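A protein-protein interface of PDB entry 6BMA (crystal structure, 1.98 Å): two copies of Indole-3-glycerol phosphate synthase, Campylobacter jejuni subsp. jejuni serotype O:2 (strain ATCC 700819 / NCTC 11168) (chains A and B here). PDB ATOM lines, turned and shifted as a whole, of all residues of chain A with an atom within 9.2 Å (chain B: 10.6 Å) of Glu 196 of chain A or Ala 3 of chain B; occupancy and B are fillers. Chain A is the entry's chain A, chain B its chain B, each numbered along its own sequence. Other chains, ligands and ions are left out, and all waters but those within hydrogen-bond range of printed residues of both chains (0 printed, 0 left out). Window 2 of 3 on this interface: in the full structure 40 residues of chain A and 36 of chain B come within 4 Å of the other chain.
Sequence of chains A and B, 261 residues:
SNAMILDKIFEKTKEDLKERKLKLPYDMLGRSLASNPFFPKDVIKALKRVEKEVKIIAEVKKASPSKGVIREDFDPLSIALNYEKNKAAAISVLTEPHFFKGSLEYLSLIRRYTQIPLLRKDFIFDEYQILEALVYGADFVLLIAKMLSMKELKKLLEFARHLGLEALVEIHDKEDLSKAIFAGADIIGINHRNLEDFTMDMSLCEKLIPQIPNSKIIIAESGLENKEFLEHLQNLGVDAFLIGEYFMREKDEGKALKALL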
ATOM      1  N   PRO A  65     -21.364  12.233  16.527  1.00  0.00           N
ATOM      2  CA  PRO A  65     -20.929  13.214  15.518  1.00  0.00           C
ATOM      3  C   PRO A  65     -20.273  14.446  16.113  1.00  0.00           C
ATOM      4  O   PRO A  65     -19.281  14.942  15.563  1.00  0.00           O
ATOM      5  CB  PRO A  65     -22.237  13.572  14.793  1.00  0.00           C
ATOM      6  CG  PRO A  65     -23.147  12.441  15.060  1.00  0.00           C
ATOM      7  CD  PRO A  65     -22.801  11.941  16.426  1.00  0.00           C
ATOM      8  N   SER A  66     -20.793  14.964  17.224  1.00  0.00           N
ATOM      9  CA  SER A  66     -20.231  16.194  17.775  1.00  0.00           C
ATOM     10  C   SER A  66     -18.968  15.947  18.591  1.00  0.00           C
ATOM     11  O   SER A  66     -18.063  16.787  18.587  1.00  0.00           O
ATOM     12  CB  SER A  66     -21.270  16.919  18.632  1.00  0.00           C
ATOM     13  OG  SER A  66     -21.657  16.155  19.758  1.00  0.00           O
ATOM     14  N   LYS A 146     -38.586  15.049  13.214  1.00  0.00           N
ATOM     15  CA  LYS A 146     -38.186  16.161  12.357  1.00  0.00           C
ATOM     16  C   LYS A 146     -37.826  15.694  10.952  1.00  0.00           C
ATOM     17  O   LYS A 146     -37.991  16.452   9.994  1.00  0.00           O
ATOM     18  CB  LYS A 146     -37.015  16.919  12.979  1.00  0.00           C
ATOM     19  CG  LYS A 146     -36.690  18.242  12.264  1.00  0.00           C
ATOM     20  CD  LYS A 146     -36.357  19.369  13.248  1.00  0.00           C
ATOM     21  CE  LYS A 146     -37.616  19.929  13.928  1.00  0.00           C
ATOM     22  NZ  LYS A 146     -38.528  20.659  12.990  1.00  0.00           N
ATOM     23  N   MET A 147     -37.367  14.454  10.803  1.00  0.00           N
ATOM     24  CA  MET A 147     -36.862  13.964   9.528  1.00  0.00           C
ATOM     25  C   MET A 147     -37.898  13.212   8.711  1.00  0.00           C
ATOM     26  O   MET A 147     -37.562  12.697   7.641  1.00  0.00           O
ATOM     27  CB  MET A 147     -35.652  13.056   9.758  1.00  0.00           C
ATOM     28  CG  MET A 147     -34.442  13.799  10.301  1.00  0.00           C
ATOM     29  SD  MET A 147     -34.001  15.305   9.386  1.00  0.00           S
ATOM     30  CE  MET A 147     -33.570  14.650   7.768  1.00  0.00           C
ATOM     31  N   GLU A 170     -38.687  10.606  18.650  1.00  0.00           N
ATOM     32  CA  GLU A 170     -37.896  11.713  19.171  1.00  0.00           C
ATOM     33  C   GLU A 170     -38.440  13.042  18.662  1.00  0.00           C
ATOM     34  O   GLU A 170     -38.683  13.195  17.462  1.00  0.00           O
ATOM     35  CB  GLU A 170     -36.444  11.536  18.747  1.00  0.00           C
ATOM     36  CG  GLU A 170     -35.559  12.711  19.063  1.00  0.00           C
ATOM     37  CD  GLU A 170     -34.110  12.396  18.781  1.00  0.00           C
ATOM     38  OE1 GLU A 170     -33.683  11.271  19.119  1.00  0.00           O
ATOM     39  OE2 GLU A 170     -33.410  13.267  18.218  1.00  0.00           O
ATOM     40  N   HIS A 172     -38.174  17.536  19.119  1.00  0.00           N
ATOM     41  CA  HIS A 172     -37.372  18.666  19.575  1.00  0.00           C
ATOM     42  C   HIS A 172     -38.168  19.948  19.750  1.00  0.00           C
ATOM     43  O   HIS A 172     -37.638  20.900  20.332  1.00  0.00           O
ATOM     44  CB  HIS A 172     -36.211  18.939  18.605  1.00  0.00           C
ATOM     45  CG  HIS A 172     -35.257  17.794  18.464  1.00  0.00           C
ATOM     46  ND1 HIS A 172     -33.915  17.900  18.764  1.00  0.00           N
ATOM     47  CD2 HIS A 172     -35.453  16.514  18.060  1.00  0.00           C
ATOM     48  CE1 HIS A 172     -33.325  16.738  18.542  1.00  0.00           C
ATOM     49  NE2 HIS A 172     -34.237  15.877  18.120  1.00  0.00           N
ATOM     50  N   ASN A 191     -35.813  15.382  23.265  1.00  0.00           N
ATOM     51  CA  ASN A 191     -34.364  15.430  23.131  1.00  0.00           C
ATOM     52  C   ASN A 191     -33.901  16.867  23.327  1.00  0.00           C
ATOM     53  O   ASN A 191     -34.301  17.759  22.571  1.00  0.00           O
ATOM     54  CB  ASN A 191     -33.935  14.902  21.766  1.00  0.00           C
ATOM     55  CG  ASN A 191     -32.441  14.678  21.671  1.00  0.00           C
ATOM     56  OD1 ASN A 191     -31.655  15.308  22.380  1.00  0.00           O
ATOM     57  ND2 ASN A 191     -32.044  13.773  20.795  1.00  0.00           N
ATOM     58  N   ARG A 193     -30.941  18.110  22.872  1.00  0.00           N
ATOM     59  CA  ARG A 193     -29.882  18.528  21.962  1.00  0.00           C
ATOM     60  C   ARG A 193     -30.459  18.867  20.591  1.00  0.00           C
ATOM     61  O   ARG A 193     -31.262  18.105  20.047  1.00  0.00           O
ATOM     62  CB  ARG A 193     -28.825  17.426  21.838  1.00  0.00           C
ATOM     63  CG  ARG A 193     -27.650  17.782  20.935  1.00  0.00           C
ATOM     64  CD  ARG A 193     -26.619  16.656  20.855  1.00  0.00           C
ATOM     65  NE  ARG A 193     -25.799  16.554  22.061  1.00  0.00           N
ATOM     66  CZ  ARG A 193     -25.890  15.571  22.955  1.00  0.00           C
ATOM     67  NH1 ARG A 193     -25.099  15.572  24.019  1.00  0.00           N
ATOM     68  NH2 ARG A 193     -26.764  14.585  22.784  1.00  0.00           N
ATOM     69  N   ASN A 194     -30.046  20.008  20.040  1.00  0.00           N
ATOM     70  CA  ASN A 194     -30.482  20.402  18.703  1.00  0.00           C
ATOM     71  C   ASN A 194     -29.840  19.499  17.655  1.00  0.00           C
ATOM     72  O   ASN A 194     -28.631  19.251  17.688  1.00  0.00           O
ATOM     73  CB  ASN A 194     -30.122  21.864  18.441  1.00  0.00           C
ATOM     74  CG  ASN A 194     -30.753  22.404  17.173  1.00  0.00           C
ATOM     75  OD1 ASN A 194     -30.843  21.712  16.159  1.00  0.00           O
ATOM     76  ND2 ASN A 194     -31.199  23.653  17.228  1.00  0.00           N
ATOM     77  N   LEU A 195     -30.651  19.036  16.704  1.00  0.00           N
ATOM     78  CA  LEU A 195     -30.232  18.004  15.764  1.00  0.00           C
ATOM     79  C   LEU A 195     -29.317  18.518  14.657  1.00  0.00           C
ATOM     80  O   LEU A 195     -28.796  17.706  13.886  1.00  0.00           O
ATOM     81  CB  LEU A 195     -31.465  17.333  15.149  1.00  0.00           C
ATOM     82  N   GLU A 196     -29.106  19.829  14.555  1.00  0.00           N
ATOM     83  CA  GLU A 196     -28.172  20.397  13.587  1.00  0.00           C
ATOM     84  C   GLU A 196     -26.967  21.063  14.228  1.00  0.00           C
ATOM     85  O   GLU A 196     -25.849  20.901  13.735  1.00  0.00           O
ATOM     86  CB  GLU A 196     -28.882  21.422  12.695  1.00  0.00           C
ATOM     87  N   ASP A 197     -27.163  21.808  15.316  1.00  0.00           N
ATOM     88  CA  ASP A 197     -26.106  22.612  15.915  1.00  0.00           C
ATOM     89  C   ASP A 197     -25.580  22.052  17.232  1.00  0.00           C
ATOM     90  O   ASP A 197     -24.663  22.645  17.814  1.00  0.00           O
ATOM     91  CB  ASP A 197     -26.598  24.049  16.130  1.00  0.00           C
ATOM     92  N   PHE A 198     -26.137  20.946  17.723  1.00  0.00           N
ATOM     93  CA  PHE A 198     -25.704  20.265  18.942  1.00  0.00           C
ATOM     94  C   PHE A 198     -25.827  21.131  20.193  1.00  0.00           C
ATOM     95  O   PHE A 198     -25.320  20.751  21.256  1.00  0.00           O
ATOM     96  CB  PHE A 198     -24.270  19.743  18.808  1.00  0.00           C
ATOM     97  CG  PHE A 198     -24.063  18.877  17.603  1.00  0.00           C
ATOM     98  CD1 PHE A 198     -24.912  17.811  17.345  1.00  0.00           C
ATOM     99  CD2 PHE A 198     -23.033  19.145  16.713  1.00  0.00           C
ATOM    100  CE1 PHE A 198     -24.727  17.017  16.233  1.00  0.00           C
ATOM    101  CE2 PHE A 198     -22.840  18.356  15.597  1.00  0.00           C
ATOM    102  CZ  PHE A 198     -23.686  17.291  15.356  1.00  0.00           C
ATOM    103  N   THR A 199     -26.492  22.278  20.099  1.00  0.00           N
ATOM    104  CA  THR A 199     -26.780  23.091  21.267  1.00  0.00           C
ATOM    105  C   THR A 199     -27.840  22.415  22.140  1.00  0.00           C
ATOM    106  O   THR A 199     -28.586  21.541  21.693  1.00  0.00           O
ATOM    107  CB  THR A 199     -27.241  24.484  20.838  1.00  0.00           C
ATOM    108  OG1 THR A 199     -28.004  24.383  19.629  1.00  0.00           O
ATOM    109  CG2 THR A 199     -26.040  25.378  20.587  1.00  0.00           C
ATOM    110  N   ALA B   3     -29.781  23.029   9.520  1.00  0.00           N
ATOM    111  CA  ALA B   3     -29.893  21.814   8.718  1.00  0.00           C
ATOM    112  C   ALA B   3     -28.520  21.377   8.216  1.00  0.00           C
ATOM    113  O   ALA B   3     -28.020  21.896   7.220  1.00  0.00           O
ATOM    114  CB  ALA B   3     -30.849  22.028   7.547  1.00  0.00           C
ATOM    115  N   MET B   4     -27.913  20.415   8.909  1.00  0.00           N
ATOM    116  CA  MET B   4     -26.559  20.001   8.568  1.00  0.00           C
ATOM    117  C   MET B   4     -26.334  18.514   8.827  1.00  0.00           C
ATOM    118  O   MET B   4     -26.376  17.697   7.901  1.00  0.00           O
ATOM    119  CB  MET B   4     -25.539  20.832   9.355  1.00  0.00           C
ATOM    120  N   ILE B   5     -26.101  18.155  10.089  1.00  0.00           N
ATOM    121  CA  ILE B   5     -25.559  16.836  10.389  1.00  0.00           C
ATOM    122  C   ILE B   5     -26.616  15.754  10.191  1.00  0.00           C
ATOM    123  O   ILE B   5     -26.319  14.666   9.680  1.00  0.00           O
ATOM    124  CB  ILE B   5     -24.971  16.824  11.810  1.00  0.00           C
ATOM    125  CG1 ILE B   5     -24.432  15.435  12.161  1.00  0.00           C
ATOM    126  CG2 ILE B   5     -25.999  17.293  12.810  1.00  0.00           C
ATOM    127  CD1 ILE B   5     -23.299  14.991  11.267  1.00  0.00           C
ATOM    128  N   LEU B   6     -27.864  16.027  10.574  1.00  0.00           N
ATOM    129  CA  LEU B   6     -28.896  15.008  10.428  1.00  0.00           C
ATOM    130  C   LEU B   6     -29.180  14.712   8.959  1.00  0.00           C
ATOM    131  O   LEU B   6     -29.468  13.563   8.604  1.00  0.00           O
ATOM    132  CB  LEU B   6     -30.166  15.436  11.160  1.00  0.00           C
ATOM    133  CG  LEU B   6     -31.152  14.319  11.503  1.00  0.00           C
ATOM    134  CD1 LEU B   6     -30.424  13.044  11.869  1.00  0.00           C
ATOM    135  CD2 LEU B   6     -32.039  14.752  12.650  1.00  0.00           C
ATOM    136  N   ASP B   7     -29.070  15.720   8.090  1.00  0.00           N
ATOM    137  CA  ASP B   7     -29.203  15.473   6.658  1.00  0.00           C
ATOM    138  C   ASP B   7     -28.037  14.647   6.127  1.00  0.00           C
ATOM    139  O   ASP B   7     -28.224  13.781   5.265  1.00  0.00           O
ATOM    140  CB  ASP B   7     -29.303  16.801   5.904  1.00  0.00           C
ATOM    141  CG  ASP B   7     -30.513  17.616   6.316  1.00  0.00           C
ATOM    142  OD1 ASP B   7     -31.649  17.115   6.181  1.00  0.00           O
ATOM    143  OD2 ASP B   7     -30.328  18.758   6.785  1.00  0.00           O
ATOM    144  N   LYS B   8     -26.820  14.918   6.608  1.00  0.00           N
ATOM    145  CA  LYS B   8     -25.664  14.123   6.206  1.00  0.00           C
ATOM    146  C   LYS B   8     -25.824  12.670   6.635  1.00  0.00           C
ATOM    147  O   LYS B   8     -25.540  11.746   5.865  1.00  0.00           O
ATOM    148  CB  LYS B   8     -24.384  14.696   6.813  1.00  0.00           C
ATOM    149  CG  LYS B   8     -23.808  15.907   6.106  1.00  0.00           C
ATOM    150  CD  LYS B   8     -22.394  16.185   6.595  1.00  0.00           C
ATOM    151  N   ILE B   9     -26.237  12.455   7.884  1.00  0.00           N
ATOM    152  CA  ILE B   9     -26.395  11.096   8.390  1.00  0.00           C
ATOM    153  C   ILE B   9     -27.438  10.351   7.569  1.00  0.00           C
ATOM    154  O   ILE B   9     -27.227   9.207   7.145  1.00  0.00           O
ATOM    155  CB  ILE B   9     -26.762  11.117   9.885  1.00  0.00           C
ATOM    156  CG1 ILE B   9     -25.652  11.768  10.708  1.00  0.00           C
ATOM    157  CG2 ILE B   9     -26.994   9.706  10.394  1.00  0.00           C
ATOM    158  CD1 ILE B   9     -25.916  11.742  12.197  1.00  0.00           C
ATOM    159  N   PHE B  10     -28.574  11.002   7.308  1.00  0.00           N
ATOM    160  CA  PHE B  10     -29.638  10.339   6.569  1.00  0.00           C
ATOM    161  C   PHE B  10     -29.192   9.984   5.157  1.00  0.00           C
ATOM    162  O   PHE B  10     -29.527   8.907   4.647  1.00  0.00           O
ATOM    163  CB  PHE B  10     -30.896  11.210   6.559  1.00  0.00           C
ATOM    164  CG  PHE B  10     -31.882  10.850   7.643  1.00  0.00           C
ATOM    165  CD1 PHE B  10     -31.743  11.355   8.926  1.00  0.00           C
ATOM    166  CD2 PHE B  10     -32.929   9.979   7.389  1.00  0.00           C
ATOM    167  CE1 PHE B  10     -32.638  11.008   9.930  1.00  0.00           C
ATOM    168  CE2 PHE B  10     -33.828   9.634   8.391  1.00  0.00           C
ATOM    169  CZ  PHE B  10     -33.679  10.156   9.662  1.00  0.00           C
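Among the printed residues, pairs that only touch across the chains: Leu 195 of chain A with Ile 5 of chain B, Met 147 of chain A with Phe 10 of chain B, Phe 198 of chain A with Ile 5 of chain B, Met 147 of chain A with Leu 6 of chain B, Met 147 of chain A with Asp 7 of chain B, Leu 195 of chain A with Leu 6 of chain B, Glu 196 of chain A with Ala 3 of chain B, Glu 196 of chain A with Ile 5 of chain B and Pro 65 of chain A with Ile 5 of chain B.
No position is printed for both chains. Of the 9 pairs that touch across the chains among the printed residues, none has its exchanged pair printed and touching as well.
Of the printed residues of chain B, Met 147 of chain A touches Leu 6 (3.5 Å), Asp 7 (3.5 Å) and Phe 10 (3.3 Å). No residue of chain B comes within 4 Å of Asn 194 of chain A. Of chain B, only Ala 3 (3.7 Å) and Ile 5 (3.7 Å) come within 4 Å of Glu 196 of chain A. No residue of chain B comes within 4 Å of Asp 197 of chain A. Of the printed residues of chain B, Phe 198 of chain A touches Ile 5 (3.4 Å). Ala 3 of chain B touches just one residue of chain A: Glu 196. Lys 8 of chain B touches none of the printed residues of chain A. The nearest residue of chain A that does not touch Ala 3 of chain B is Asp 197 of chain A (6.5 Å). The nearest printed residue of chain B that does not touch Pro 65 of chain A is Ile 9 of chain B (4.04 Å).
N of Glu 196 of chain A sits at hydrogen-bond distance from OD1 of Asn 194 of chain A (3.0 Å).
Of the 14 printed residues of chain A, 5 touch a printed residue of chain B. Hydrophobic or aromatic side chains of chain A within 4 Å of the printed part of chain B: Pro 65, Met 147, Leu 195 and Phe 198. Along chain A the printed residues that touch a printed residue of chain B span positions 65 to 198. Of the 8 printed residues of chain B, 5 touch a printed residue of chain A. Printed residues of chain B that touch a printed residue of chain A: Ala 3, Ile 5, Leu 6, Asp 7 and Phe 10. Hydrophobic or aromatic side chains of chain B that line the printed part of chain A: Ile 5, Leu 6 and Phe 10. Among the printed residues, 9 pairs touch across the chains. Among the printed residues, no Asp or Glu carboxylate lies within 4 Å of a Lys or Arg side-chain nitrogen of the other chain.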
